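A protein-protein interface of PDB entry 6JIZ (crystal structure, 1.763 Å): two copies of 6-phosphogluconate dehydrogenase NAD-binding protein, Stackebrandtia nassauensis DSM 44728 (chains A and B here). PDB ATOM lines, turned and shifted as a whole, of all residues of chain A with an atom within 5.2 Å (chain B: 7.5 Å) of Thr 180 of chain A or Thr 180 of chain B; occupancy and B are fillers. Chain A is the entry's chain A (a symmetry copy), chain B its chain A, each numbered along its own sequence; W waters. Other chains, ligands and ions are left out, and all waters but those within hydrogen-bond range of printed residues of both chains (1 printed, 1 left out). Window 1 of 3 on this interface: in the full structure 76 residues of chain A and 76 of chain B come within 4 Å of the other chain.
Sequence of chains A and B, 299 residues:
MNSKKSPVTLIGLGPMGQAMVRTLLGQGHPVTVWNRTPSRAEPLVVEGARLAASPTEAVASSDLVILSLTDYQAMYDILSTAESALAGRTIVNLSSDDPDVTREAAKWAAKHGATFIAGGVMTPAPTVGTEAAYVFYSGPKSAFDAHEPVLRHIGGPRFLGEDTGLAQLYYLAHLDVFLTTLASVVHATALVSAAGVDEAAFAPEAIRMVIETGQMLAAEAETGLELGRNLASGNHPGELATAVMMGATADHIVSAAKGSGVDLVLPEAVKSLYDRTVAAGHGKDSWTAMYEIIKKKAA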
ATOM      1  N   LEU A 175     -23.324 -11.434 -19.648  1.00  0.00           N
ATOM      2  CA  LEU A 175     -22.765 -10.906 -18.403  1.00  0.00           C
ATOM      3  C   LEU A 175     -21.368 -10.328 -18.598  1.00  0.00           C
ATOM      4  O   LEU A 175     -20.955  -9.469 -17.813  1.00  0.00           O
ATOM      5  CB  LEU A 175     -22.750 -12.003 -17.331  1.00  0.00           C
ATOM      6  CG  LEU A 175     -24.012 -12.059 -16.460  1.00  0.00           C
ATOM      7  CD1 LEU A 175     -24.040 -10.899 -15.457  1.00  0.00           C
ATOM      8  CD2 LEU A 175     -25.293 -12.076 -17.281  1.00  0.00           C
ATOM      9  N   ASP A 176     -20.642 -10.794 -19.621  1.00  0.00           N
ATOM     10  CA  ASP A 176     -19.377 -10.198 -20.049  1.00  0.00           C
ATOM     11  C   ASP A 176     -19.573  -8.709 -20.348  1.00  0.00           C
ATOM     12  O   ASP A 176     -18.855  -7.848 -19.821  1.00  0.00           O
ATOM     13  CB  ASP A 176     -18.910 -10.974 -21.294  1.00  0.00           C
ATOM     14  CG  ASP A 176     -17.482 -10.687 -21.724  1.00  0.00           C
ATOM     15  OD1 ASP A 176     -16.786  -9.851 -21.114  1.00  0.00           O
ATOM     16  OD2 ASP A 176     -17.059 -11.333 -22.716  1.00  0.00           O
ATOM     17  N   VAL A 177     -20.586  -8.391 -21.156  1.00  0.00           N
ATOM     18  CA  VAL A 177     -20.902  -6.989 -21.445  1.00  0.00           C
ATOM     19  C   VAL A 177     -21.319  -6.268 -20.166  1.00  0.00           C
ATOM     20  O   VAL A 177     -20.817  -5.182 -19.854  1.00  0.00           O
ATOM     21  CB  VAL A 177     -21.997  -6.895 -22.524  1.00  0.00           C
ATOM     22  CG1 VAL A 177     -22.366  -5.436 -22.811  1.00  0.00           C
ATOM     23  CG2 VAL A 177     -21.539  -7.589 -23.816  1.00  0.00           C
ATOM     24  N   PHE A 178     -22.243  -6.871 -19.409  1.00  0.00           N
ATOM     25  CA  PHE A 178     -22.796  -6.256 -18.197  1.00  0.00           C
ATOM     26  C   PHE A 178     -21.703  -5.911 -17.185  1.00  0.00           C
ATOM     27  O   PHE A 178     -21.572  -4.758 -16.759  1.00  0.00           O
ATOM     28  CB  PHE A 178     -23.830  -7.217 -17.587  1.00  0.00           C
ATOM     29  CG  PHE A 178     -24.650  -6.637 -16.456  1.00  0.00           C
ATOM     30  CD1 PHE A 178     -25.566  -5.619 -16.688  1.00  0.00           C
ATOM     31  CD2 PHE A 178     -24.539  -7.155 -15.172  1.00  0.00           C
ATOM     32  CE1 PHE A 178     -26.353  -5.111 -15.655  1.00  0.00           C
ATOM     33  CE2 PHE A 178     -25.328  -6.654 -14.124  1.00  0.00           C
ATOM     34  CZ  PHE A 178     -26.224  -5.627 -14.373  1.00  0.00           C
ATOM     35  N   LEU A 179     -20.911  -6.901 -16.774  1.00  0.00           N
ATOM     36  CA  LEU A 179     -19.938  -6.664 -15.709  1.00  0.00           C
ATOM     37  C   LEU A 179     -18.848  -5.695 -16.154  1.00  0.00           C
ATOM     38  O   LEU A 179     -18.383  -4.864 -15.362  1.00  0.00           O
ATOM     39  CB  LEU A 179     -19.303  -7.978 -15.260  1.00  0.00           C
ATOM     40  CG  LEU A 179     -20.240  -8.997 -14.602  1.00  0.00           C
ATOM     41  CD1 LEU A 179     -19.433 -10.195 -14.119  1.00  0.00           C
ATOM     42  CD2 LEU A 179     -21.023  -8.370 -13.464  1.00  0.00           C
ATOM     43  N   THR A 180     -18.419  -5.803 -17.412  1.00  0.00           N
ATOM     44  CA  THR A 180     -17.325  -4.958 -17.886  1.00  0.00           C
ATOM     45  C   THR A 180     -17.790  -3.521 -18.046  1.00  0.00           C
ATOM     46  O   THR A 180     -17.059  -2.582 -17.699  1.00  0.00           O
ATOM     47  CB  THR A 180     -16.767  -5.488 -19.213  1.00  0.00           C
ATOM     48  OG1 THR A 180     -16.465  -6.886 -19.089  1.00  0.00           O
ATOM     49  CG2 THR A 180     -15.457  -4.732 -19.586  1.00  0.00           C
ATOM     50  N   THR A 181     -18.997  -3.337 -18.579  1.00  0.00           N
ATOM     51  CA  THR A 181     -19.573  -2.002 -18.717  1.00  0.00           C
ATOM     52  C   THR A 181     -19.764  -1.357 -17.353  1.00  0.00           C
ATOM     53  O   THR A 181     -19.391  -0.196 -17.145  1.00  0.00           O
ATOM     54  CB  THR A 181     -20.898  -2.096 -19.470  1.00  0.00           C
ATOM     55  OG1 THR A 181     -20.650  -2.620 -20.785  1.00  0.00           O
ATOM     56  CG2 THR A 181     -21.582  -0.732 -19.550  1.00  0.00           C
ATOM     57  N   LEU A 182     -20.296  -2.115 -16.393  1.00  0.00           N
ATOM     58  CA  LEU A 182     -20.477  -1.574 -15.047  1.00  0.00           C
ATOM     59  C   LEU A 182     -19.142  -1.209 -14.401  1.00  0.00           C
ATOM     60  O   LEU A 182     -19.040  -0.177 -13.725  1.00  0.00           O
ATOM     61  CB  LEU A 182     -21.226  -2.588 -14.180  1.00  0.00           C
ATOM     62  CG  LEU A 182     -22.702  -2.816 -14.501  1.00  0.00           C
ATOM     63  CD1 LEU A 182     -23.286  -3.825 -13.504  1.00  0.00           C
ATOM     64  CD2 LEU A 182     -23.453  -1.521 -14.421  1.00  0.00           C
ATOM     65  N   ALA A 183     -18.115  -2.052 -14.564  1.00  0.00           N
ATOM     66  CA  ALA A 183     -16.811  -1.731 -13.990  1.00  0.00           C
ATOM     67  C   ALA A 183     -16.269  -0.430 -14.574  1.00  0.00           C
ATOM     68  O   ALA A 183     -15.640   0.366 -13.862  1.00  0.00           O
ATOM     69  CB  ALA A 183     -15.811  -2.867 -14.228  1.00  0.00           C
ATOM     70  N   SER A 184     -16.522  -0.188 -15.865  1.00  0.00           N
ATOM     71  CA  SER A 184     -15.996   1.020 -16.497  1.00  0.00           C
ATOM     72  C   SER A 184     -16.679   2.276 -15.970  1.00  0.00           C
ATOM     73  O   SER A 184     -16.035   3.326 -15.869  1.00  0.00           O
ATOM     74  CB  SER A 184     -16.125   0.936 -18.023  1.00  0.00           C
ATOM     75  OG  SER A 184     -17.430   1.270 -18.483  1.00  0.00           O
ATOM     76  N   LEU A 266      -8.041  -2.299 -15.496  1.00  0.00           N
ATOM     77  CA  LEU A 266      -9.071  -2.208 -16.533  1.00  0.00           C
ATOM     78  C   LEU A 266      -8.595  -1.380 -17.726  1.00  0.00           C
ATOM     79  O   LEU A 266      -8.645  -1.890 -18.862  1.00  0.00           O
ATOM     80  CB  LEU A 266     -10.387  -1.684 -15.933  1.00  0.00           C
ATOM     81  CG  LEU A 266     -11.650  -1.799 -16.797  1.00  0.00           C
ATOM     82  CD1 LEU A 266     -11.978  -3.284 -17.030  1.00  0.00           C
ATOM     83  CD2 LEU A 266     -12.862  -1.094 -16.176  1.00  0.00           C
ATOM     84  N   VAL A 270      -7.739  -2.563 -21.924  1.00  0.00           N
ATOM     85  CA  VAL A 270      -8.203  -1.922 -23.151  1.00  0.00           C
ATOM     86  C   VAL A 270      -7.013  -1.485 -23.993  1.00  0.00           C
ATOM     87  O   VAL A 270      -6.972  -1.713 -25.210  1.00  0.00           O
ATOM     88  CB  VAL A 270      -9.131  -0.736 -22.815  1.00  0.00           C
ATOM     89  CG1 VAL A 270      -9.453   0.080 -24.073  1.00  0.00           C
ATOM     90  CG2 VAL A 270     -10.438  -1.222 -22.131  1.00  0.00           C
ATOM     91  N   HIS B 174     -15.214   9.914 -19.866  1.00  0.00           N
ATOM     92  CA  HIS B 174     -16.292   9.479 -20.757  1.00  0.00           C
ATOM     93  C   HIS B 174     -15.786   8.433 -21.744  1.00  0.00           C
ATOM     94  O   HIS B 174     -16.457   7.423 -21.995  1.00  0.00           O
ATOM     95  CB  HIS B 174     -16.888  10.668 -21.524  1.00  0.00           C
ATOM     96  CG  HIS B 174     -17.906  11.459 -20.757  1.00  0.00           C
ATOM     97  ND1 HIS B 174     -17.577  12.265 -19.686  1.00  0.00           N
ATOM     98  CD2 HIS B 174     -19.245  11.586 -20.923  1.00  0.00           C
ATOM     99  CE1 HIS B 174     -18.672  12.839 -19.215  1.00  0.00           C
ATOM    100  NE2 HIS B 174     -19.696  12.452 -19.957  1.00  0.00           N
ATOM    101  N   LEU B 175     -14.600   8.656 -22.318  1.00  0.00           N
ATOM    102  CA  LEU B 175     -14.056   7.687 -23.272  1.00  0.00           C
ATOM    103  C   LEU B 175     -13.640   6.385 -22.598  1.00  0.00           C
ATOM    104  O   LEU B 175     -13.602   5.347 -23.264  1.00  0.00           O
ATOM    105  CB  LEU B 175     -12.873   8.306 -24.027  1.00  0.00           C
ATOM    106  CG  LEU B 175     -13.255   9.020 -25.332  1.00  0.00           C
ATOM    107  CD1 LEU B 175     -13.595   8.006 -26.433  1.00  0.00           C
ATOM    108  CD2 LEU B 175     -14.400  10.005 -25.152  1.00  0.00           C
ATOM    109  N   ASP B 176     -13.321   6.435 -21.299  1.00  0.00           N
ATOM    110  CA  ASP B 176     -13.100   5.245 -20.478  1.00  0.00           C
ATOM    111  C   ASP B 176     -14.318   4.321 -20.553  1.00  0.00           C
ATOM    112  O   ASP B 176     -14.200   3.127 -20.859  1.00  0.00           O
ATOM    113  CB  ASP B 176     -12.837   5.730 -19.041  1.00  0.00           C
ATOM    114  CG  ASP B 176     -12.313   4.663 -18.095  1.00  0.00           C
ATOM    115  OD1 ASP B 176     -12.157   3.488 -18.481  1.00  0.00           O
ATOM    116  OD2 ASP B 176     -12.053   5.037 -16.923  1.00  0.00           O
ATOM    117  N   VAL B 177     -15.506   4.882 -20.327  1.00  0.00           N
ATOM    118  CA  VAL B 177     -16.740   4.098 -20.447  1.00  0.00           C
ATOM    119  C   VAL B 177     -16.920   3.616 -21.884  1.00  0.00           C
ATOM    120  O   VAL B 177     -17.176   2.432 -22.131  1.00  0.00           O
ATOM    121  CB  VAL B 177     -17.951   4.925 -19.976  1.00  0.00           C
ATOM    122  CG1 VAL B 177     -19.253   4.133 -20.131  1.00  0.00           C
ATOM    123  CG2 VAL B 177     -17.768   5.363 -18.515  1.00  0.00           C
ATOM    124  N   PHE B 178     -16.783   4.533 -22.848  1.00  0.00           N
ATOM    125  CA  PHE B 178     -17.009   4.228 -24.265  1.00  0.00           C
ATOM    126  C   PHE B 178     -16.112   3.089 -24.752  1.00  0.00           C
ATOM    127  O   PHE B 178     -16.596   2.077 -25.272  1.00  0.00           O
ATOM    128  CB  PHE B 178     -16.770   5.507 -25.086  1.00  0.00           C
ATOM    129  CG  PHE B 178     -17.175   5.416 -26.540  1.00  0.00           C
ATOM    130  CD1 PHE B 178     -18.511   5.297 -26.903  1.00  0.00           C
ATOM    131  CD2 PHE B 178     -16.217   5.508 -27.542  1.00  0.00           C
ATOM    132  CE1 PHE B 178     -18.891   5.256 -28.244  1.00  0.00           C
ATOM    133  CE2 PHE B 178     -16.587   5.469 -28.896  1.00  0.00           C
ATOM    134  CZ  PHE B 178     -17.924   5.333 -29.237  1.00  0.00           C
ATOM    135  N   LEU B 179     -14.795   3.238 -24.606  1.00  0.00           N
ATOM    136  CA  LEU B 179     -13.881   2.248 -25.173  1.00  0.00           C
ATOM    137  C   LEU B 179     -14.018   0.898 -24.476  1.00  0.00           C
ATOM    138  O   LEU B 179     -13.926  -0.155 -25.122  1.00  0.00           O
ATOM    139  CB  LEU B 179     -12.436   2.731 -25.073  1.00  0.00           C
ATOM    140  CG  LEU B 179     -12.080   3.982 -25.884  1.00  0.00           C
ATOM    141  CD1 LEU B 179     -10.587   4.262 -25.760  1.00  0.00           C
ATOM    142  CD2 LEU B 179     -12.489   3.831 -27.337  1.00  0.00           C
ATOM    143  N   THR B 180     -14.221   0.915 -23.158  1.00  0.00           N
ATOM    144  CA  THR B 180     -14.286  -0.340 -22.413  1.00  0.00           C
ATOM    145  C   THR B 180     -15.580  -1.075 -22.718  1.00  0.00           C
ATOM    146  O   THR B 180     -15.582  -2.305 -22.872  1.00  0.00           O
ATOM    147  CB  THR B 180     -14.162  -0.083 -20.906  1.00  0.00           C
ATOM    148  OG1 THR B 180     -13.012   0.735 -20.646  1.00  0.00           O
ATOM    149  CG2 THR B 180     -13.991  -1.430 -20.142  1.00  0.00           C
ATOM    150  N   THR B 181     -16.685  -0.335 -22.796  1.00  0.00           N
ATOM    151  CA  THR B 181     -17.973  -0.927 -23.149  1.00  0.00           C
ATOM    152  C   THR B 181     -17.926  -1.514 -24.551  1.00  0.00           C
ATOM    153  O   THR B 181     -18.357  -2.652 -24.775  1.00  0.00           O
ATOM    154  CB  THR B 181     -19.067   0.132 -23.035  1.00  0.00           C
ATOM    155  OG1 THR B 181     -19.136   0.585 -21.672  1.00  0.00           O
ATOM    156  CG2 THR B 181     -20.416  -0.420 -23.492  1.00  0.00           C
ATOM    157  N   LEU B 182     -17.354  -0.772 -25.501  1.00  0.00           N
ATOM    158  CA  LEU B 182     -17.241  -1.286 -26.864  1.00  0.00           C
ATOM    159  C   LEU B 182     -16.364  -2.535 -26.927  1.00  0.00           C
ATOM    160  O   LEU B 182     -16.679  -3.481 -27.659  1.00  0.00           O
ATOM    161  CB  LEU B 182     -16.680  -0.197 -27.781  1.00  0.00           C
ATOM    162  CG  LEU B 182     -17.595   0.987 -28.092  1.00  0.00           C
ATOM    163  CD1 LEU B 182     -16.878   1.942 -29.053  1.00  0.00           C
ATOM    164  CD2 LEU B 182     -18.873   0.501 -28.708  1.00  0.00           C
ATOM    165  N   ALA B 183     -15.242  -2.548 -26.196  1.00  0.00           N
ATOM    166  CA  ALA B 183     -14.385  -3.733 -26.199  1.00  0.00           C
ATOM    167  C   ALA B 183     -15.142  -4.948 -25.672  1.00  0.00           C
ATOM    168  O   ALA B 183     -14.959  -6.068 -26.170  1.00  0.00           O
ATOM    169  CB  ALA B 183     -13.123  -3.499 -25.364  1.00  0.00           C
ATOM    170  N   SER B 184     -16.012  -4.742 -24.678  1.00  0.00           N
ATOM    171  CA  SER B 184     -16.739  -5.870 -24.099  1.00  0.00           C
ATOM    172  C   SER B 184     -17.757  -6.446 -25.075  1.00  0.00           C
ATOM    173  O   SER B 184     -17.992  -7.660 -25.067  1.00  0.00           O
ATOM    174  CB  SER B 184     -17.421  -5.462 -22.787  1.00  0.00           C
ATOM    175  OG  SER B 184     -18.653  -4.782 -22.997  1.00  0.00           O
ATOM    176  N   VAL B 185     -18.373  -5.608 -25.913  1.00  0.00           N
ATOM    177  CA  VAL B 185     -19.285  -6.118 -26.941  1.00  0.00           C
ATOM    178  C   VAL B 185     -18.536  -7.016 -27.923  1.00  0.00           C
ATOM    179  O   VAL B 185     -19.020  -8.092 -28.302  1.00  0.00           O
ATOM    180  CB  VAL B 185     -19.988  -4.950 -27.660  1.00  0.00           C
ATOM    181  CG1 VAL B 185     -20.771  -5.458 -28.852  1.00  0.00           C
ATOM    182  CG2 VAL B 185     -20.912  -4.239 -26.699  1.00  0.00           C
ATOM    183  N   VAL B 186     -17.334  -6.605 -28.331  1.00  0.00           N
ATOM    184  CA  VAL B 186     -16.553  -7.425 -29.247  1.00  0.00           C
ATOM    185  C   VAL B 186     -16.083  -8.695 -28.554  1.00  0.00           C
ATOM    186  O   VAL B 186     -16.092  -9.779 -29.145  1.00  0.00           O
ATOM    187  CB  VAL B 186     -15.371  -6.617 -29.813  1.00  0.00           C
ATOM    188  CG1 VAL B 186     -14.509  -7.478 -30.709  1.00  0.00           C
ATOM    189  CG2 VAL B 186     -15.889  -5.408 -30.578  1.00  0.00           C
ATOM    190  N   HIS B 187     -15.666  -8.584 -27.291  1.00  0.00           N
ATOM    191  CA  HIS B 187     -15.185  -9.761 -26.572  1.00  0.00           C
ATOM    192  C   HIS B 187     -16.304 -10.784 -26.388  1.00  0.00           C
ATOM    193  O   HIS B 187     -16.111 -11.995 -26.599  1.00  0.00           O
ATOM    194  CB  HIS B 187     -14.612  -9.345 -25.213  1.00  0.00           C
ATOM    195  CG  HIS B 187     -13.913 -10.464 -24.510  1.00  0.00           C
ATOM    196  ND1 HIS B 187     -14.563 -11.320 -23.646  1.00  0.00           N
ATOM    197  CD2 HIS B 187     -12.631 -10.896 -24.578  1.00  0.00           C
ATOM    198  CE1 HIS B 187     -13.710 -12.229 -23.208  1.00  0.00           C
ATOM    199  NE2 HIS B 187     -12.529 -11.993 -23.756  1.00  0.00           N
ATOM    200  N   THR B 213     -28.114  -2.427 -19.929  1.00  0.00           N
ATOM    201  CA  THR B 213     -27.297  -2.015 -18.793  1.00  0.00           C
ATOM    202  C   THR B 213     -27.508  -0.538 -18.489  1.00  0.00           C
ATOM    203  O   THR B 213     -27.623  -0.145 -17.319  1.00  0.00           O
ATOM    204  CB  THR B 213     -25.819  -2.297 -19.074  1.00  0.00           C
ATOM    205  OG1 THR B 213     -25.647  -3.690 -19.354  1.00  0.00           O
ATOM    206  CG2 THR B 213     -24.954  -1.924 -17.870  1.00  0.00           C
ATOM    207  N   ILE B 253     -16.793 -16.334 -16.585  1.00  0.00           N
ATOM    208  CA  ILE B 253     -16.452 -15.745 -17.876  1.00  0.00           C
ATOM    209  C   ILE B 253     -14.990 -16.016 -18.222  1.00  0.00           C
ATOM    210  O   ILE B 253     -14.666 -16.346 -19.369  1.00  0.00           O
ATOM    211  CB  ILE B 253     -16.768 -14.238 -17.876  1.00  0.00           C
ATOM    212  CG1 ILE B 253     -18.271 -14.023 -17.692  1.00  0.00           C
ATOM    213  CG2 ILE B 253     -16.259 -13.573 -19.184  1.00  0.00           C
ATOM    214  CD1 ILE B 253     -18.647 -12.601 -17.273  1.00  0.00           C
ATOM    215  N   LEU B 266      -9.163  -8.750 -20.998  1.00  0.00           N
ATOM    216  CA  LEU B 266     -10.314  -7.970 -20.538  1.00  0.00           C
ATOM    217  C   LEU B 266     -11.066  -8.689 -19.417  1.00  0.00           C
ATOM    218  O   LEU B 266     -11.254  -8.084 -18.344  1.00  0.00           O
ATOM    219  CB  LEU B 266     -11.223  -7.608 -21.724  1.00  0.00           C
ATOM    220  CG  LEU B 266     -12.311  -6.553 -21.482  1.00  0.00           C
ATOM    221  CD1 LEU B 266     -11.652  -5.200 -21.162  1.00  0.00           C
ATOM    222  CD2 LEU B 266     -13.263  -6.395 -22.674  1.00  0.00           C
ATOM    223  N   PRO B 267     -11.501  -9.951 -19.568  1.00  0.00           N
ATOM    224  CA  PRO B 267     -12.209 -10.592 -18.441  1.00  0.00           C
ATOM    225  C   PRO B 267     -11.322 -10.813 -17.227  1.00  0.00           C
ATOM    226  O   PRO B 267     -11.827 -10.827 -16.095  1.00  0.00           O
ATOM    227  CB  PRO B 267     -12.713 -11.921 -19.038  1.00  0.00           C
ATOM    228  CG  PRO B 267     -11.787 -12.200 -20.197  1.00  0.00           C
ATOM    229  CD  PRO B 267     -11.491 -10.815 -20.767  1.00  0.00           C
ATOM    230  N   ALA B 269      -9.133  -8.654 -16.161  1.00  0.00           N
ATOM    231  CA  ALA B 269      -9.160  -7.376 -15.453  1.00  0.00           C
ATOM    232  C   ALA B 269     -10.410  -7.251 -14.589  1.00  0.00           C
ATOM    233  O   ALA B 269     -10.342  -6.793 -13.442  1.00  0.00           O
ATOM    234  CB  ALA B 269      -9.088  -6.216 -16.452  1.00  0.00           C
ATOM    235  N   VAL B 270     -11.565  -7.649 -15.124  1.00  0.00           N
ATOM    236  CA  VAL B 270     -12.799  -7.610 -14.347  1.00  0.00           C
ATOM    237  C   VAL B 270     -12.698  -8.564 -13.164  1.00  0.00           C
ATOM    238  O   VAL B 270     -13.048  -8.213 -12.028  1.00  0.00           O
ATOM    239  CB  VAL B 270     -14.007  -7.945 -15.246  1.00  0.00           C
ATOM    240  CG1 VAL B 270     -15.279  -8.125 -14.410  1.00  0.00           C
ATOM    241  CG2 VAL B 270     -14.217  -6.852 -16.332  1.00  0.00           C
ATOM    242  N   LEU B 273     -10.660  -7.085 -10.364  1.00  0.00           N
ATOM    243  CA  LEU B 273     -11.406  -6.131  -9.549  1.00  0.00           C
ATOM    244  C   LEU B 273     -12.273  -6.842  -8.521  1.00  0.00           C
ATOM    245  O   LEU B 273     -12.300  -6.454  -7.347  1.00  0.00           O
ATOM    246  CB  LEU B 273     -12.271  -5.235 -10.435  1.00  0.00           C
ATOM    247  CG  LEU B 273     -11.459  -4.298 -11.340  1.00  0.00           C
ATOM    248  CD1 LEU B 273     -12.395  -3.578 -12.302  1.00  0.00           C
ATOM    249  CD2 LEU B 273     -10.681  -3.314 -10.484  1.00  0.00           C
ATOM    250  N   TYR B 274     -13.000  -7.874  -8.945  1.00  0.00           N
ATOM    251  CA  TYR B 274     -13.874  -8.588  -8.020  1.00  0.00           C
ATOM    252  C   TYR B 274     -13.068  -9.377  -7.001  1.00  0.00           C
ATOM    253  O   TYR B 274     -13.416  -9.396  -5.814  1.00  0.00           O
ATOM    254  CB  TYR B 274     -14.826  -9.502  -8.792  1.00  0.00           C
ATOM    255  CG  TYR B 274     -16.020  -8.753  -9.314  1.00  0.00           C
ATOM    256  CD1 TYR B 274     -17.041  -8.372  -8.452  1.00  0.00           C
ATOM    257  CD2 TYR B 274     -16.117  -8.395 -10.655  1.00  0.00           C
ATOM    258  CE1 TYR B 274     -18.127  -7.663  -8.903  1.00  0.00           C
ATOM    259  CE2 TYR B 274     -17.204  -7.680 -11.127  1.00  0.00           C
ATOM    260  CZ  TYR B 274     -18.207  -7.319 -10.243  1.00  0.00           C
ATOM    261  OH  TYR B 274     -19.288  -6.611 -10.679  1.00  0.00           O
HETATM  262  O   HOH W   1     -18.843  -4.875 -12.682  1.00  0.00           O
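Water W1 lies within hydrogen-bond range of OH of Tyr 274 of chain B, O of Leu 179 of chain A and N of Ala 183 of chain A.
Of the 22 printed residues of chain B, 10 touch a printed residue of chain A. Of the 12 printed residues of chain A, 11 touch a printed residue of chain B. Among the printed residues, 18 pairs touch across the chains.
ND1 of His 187 of chain B sits at hydrogen-bond distance from OD2 of Asp 176 of chain A (2.7 Å).
Among the printed residues, pairs that only touch across the chains: Phe 178 of chain A with Thr 213 of chain B (3.3 Å), Thr 181 of chain A with Thr 181 of chain B (3.5 Å), Ser 184 of chain A with Val 177 of chain B (3.5 Å), Val 177 of chain A with Ser 184 of chain B (3.5 Å), Thr 180 of chain A with Val 270 of chain B (3.6 Å), Val 270 of chain A with Thr 180 of chain B (3.6 Å), Asp 176 of chain A with Ile 253 of chain B (3.6 Å), Thr 180 of chain A with Ser 184 of chain B (3.6 Å), Ser 184 of chain A with Thr 180 of chain B (3.6 Å), Thr 180 of chain A with Thr 180 of chain B (3.7 Å), Ser 184 of chain A with Thr 181 of chain B (3.7 Å), Thr 181 of chain A with Ser 184 of chain B (3.7 Å), Leu 179 of chain A with Tyr 274 of chain B (3.7 Å), Leu 182 of chain A with Thr 213 of chain B (3.8 Å), Leu 175 of chain A with Ile 253 of chain B (3.8 Å), Thr 181 of chain A with Thr 213 of chain B (3.95 Å) and Ala 183 of chain A with Leu 273 of chain B (3.99 Å).
Thr 180 of chain A touches Ser 184 of chain B, and with the chains exchanged Ser 184 of chain A touches Thr 180 of chain B. Thr 180 of chain A touches Val 270 of chain B, and with the chains exchanged Val 270 of chain A touches Thr 180 of chain B. Thr 181 of chain A touches its own counterpart, Thr 181 of chain B. Thr 181 of chain A touches Ser 184 of chain B, and with the chains exchanged Ser 184 of chain A touches Thr 181 of chain B. 12 positions are printed for both chains.
The side-chain hydroxyl (OG1) of Thr 180 of chain B lies within hydrogen-bond range of the backbone carbonyl oxygen (O) of Asp 176 of chain B (2.7 Å). The side-chain hydroxyl of Thr 181 of chain B sits at hydrogen-bond distance from the backbone carbonyl oxygen of Val 177 of chain B. OG of Ser 184 of chain B lies within hydrogen-bond range of O of Thr 181 of chain B, 2.8 Å away. The backbone carbonyl oxygen of Asp 176 of chain A is in hydrogen-bond range of the side-chain hydroxyl of Thr 180 of chain A, at 2.7 Å. The backbone carbonyl oxygen of Val 177 of chain A lies within hydrogen-bond range of the side-chain hydroxyl of Thr 181 of chain A (2.7 Å). The backbone carbonyl oxygen (O) of Thr 181 of chain A sits at hydrogen-bond distance from the side-chain hydroxyl (OG) of Ser 184 of chain A (2.8 Å).
Of chain B, only Thr 180 (3.7 Å), Ser 184 (3.6 Å) and Val 270 (3.6 Å) come within 4 Å of Thr 180 of chain A. Of chain A, only Thr 180 (3.7 Å), Ser 184 (3.6 Å) and Val 270 (3.6 Å) come within 4 Å of Thr 180 of chain B. Of the printed residues of chain B, Ala 183 of chain A touches Leu 273. Of the printed residues of chain A, Val 270 of chain B touches Thr 180. Printed residues of chain B within 4 Å of Leu 179 of chain A: Tyr 274. Of the printed residues of chain A, Thr 213 of chain B touches Phe 178 (3.3 Å), Thr 181 (3.95 Å) and Leu 182 (3.8 Å). Of the printed residues of chain A, His 187 of chain B touches Asp 176 (2.7 Å). Phe 178 of chain B touches none of the printed residues of chain A. The nearest residue of chain B that does not touch Thr 180 of chain A is Leu 266 of chain B (4.1 Å). The nearest printed residue of chain A that does not touch Val 177 of chain B is Thr 181 of chain A (5.3 Å).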
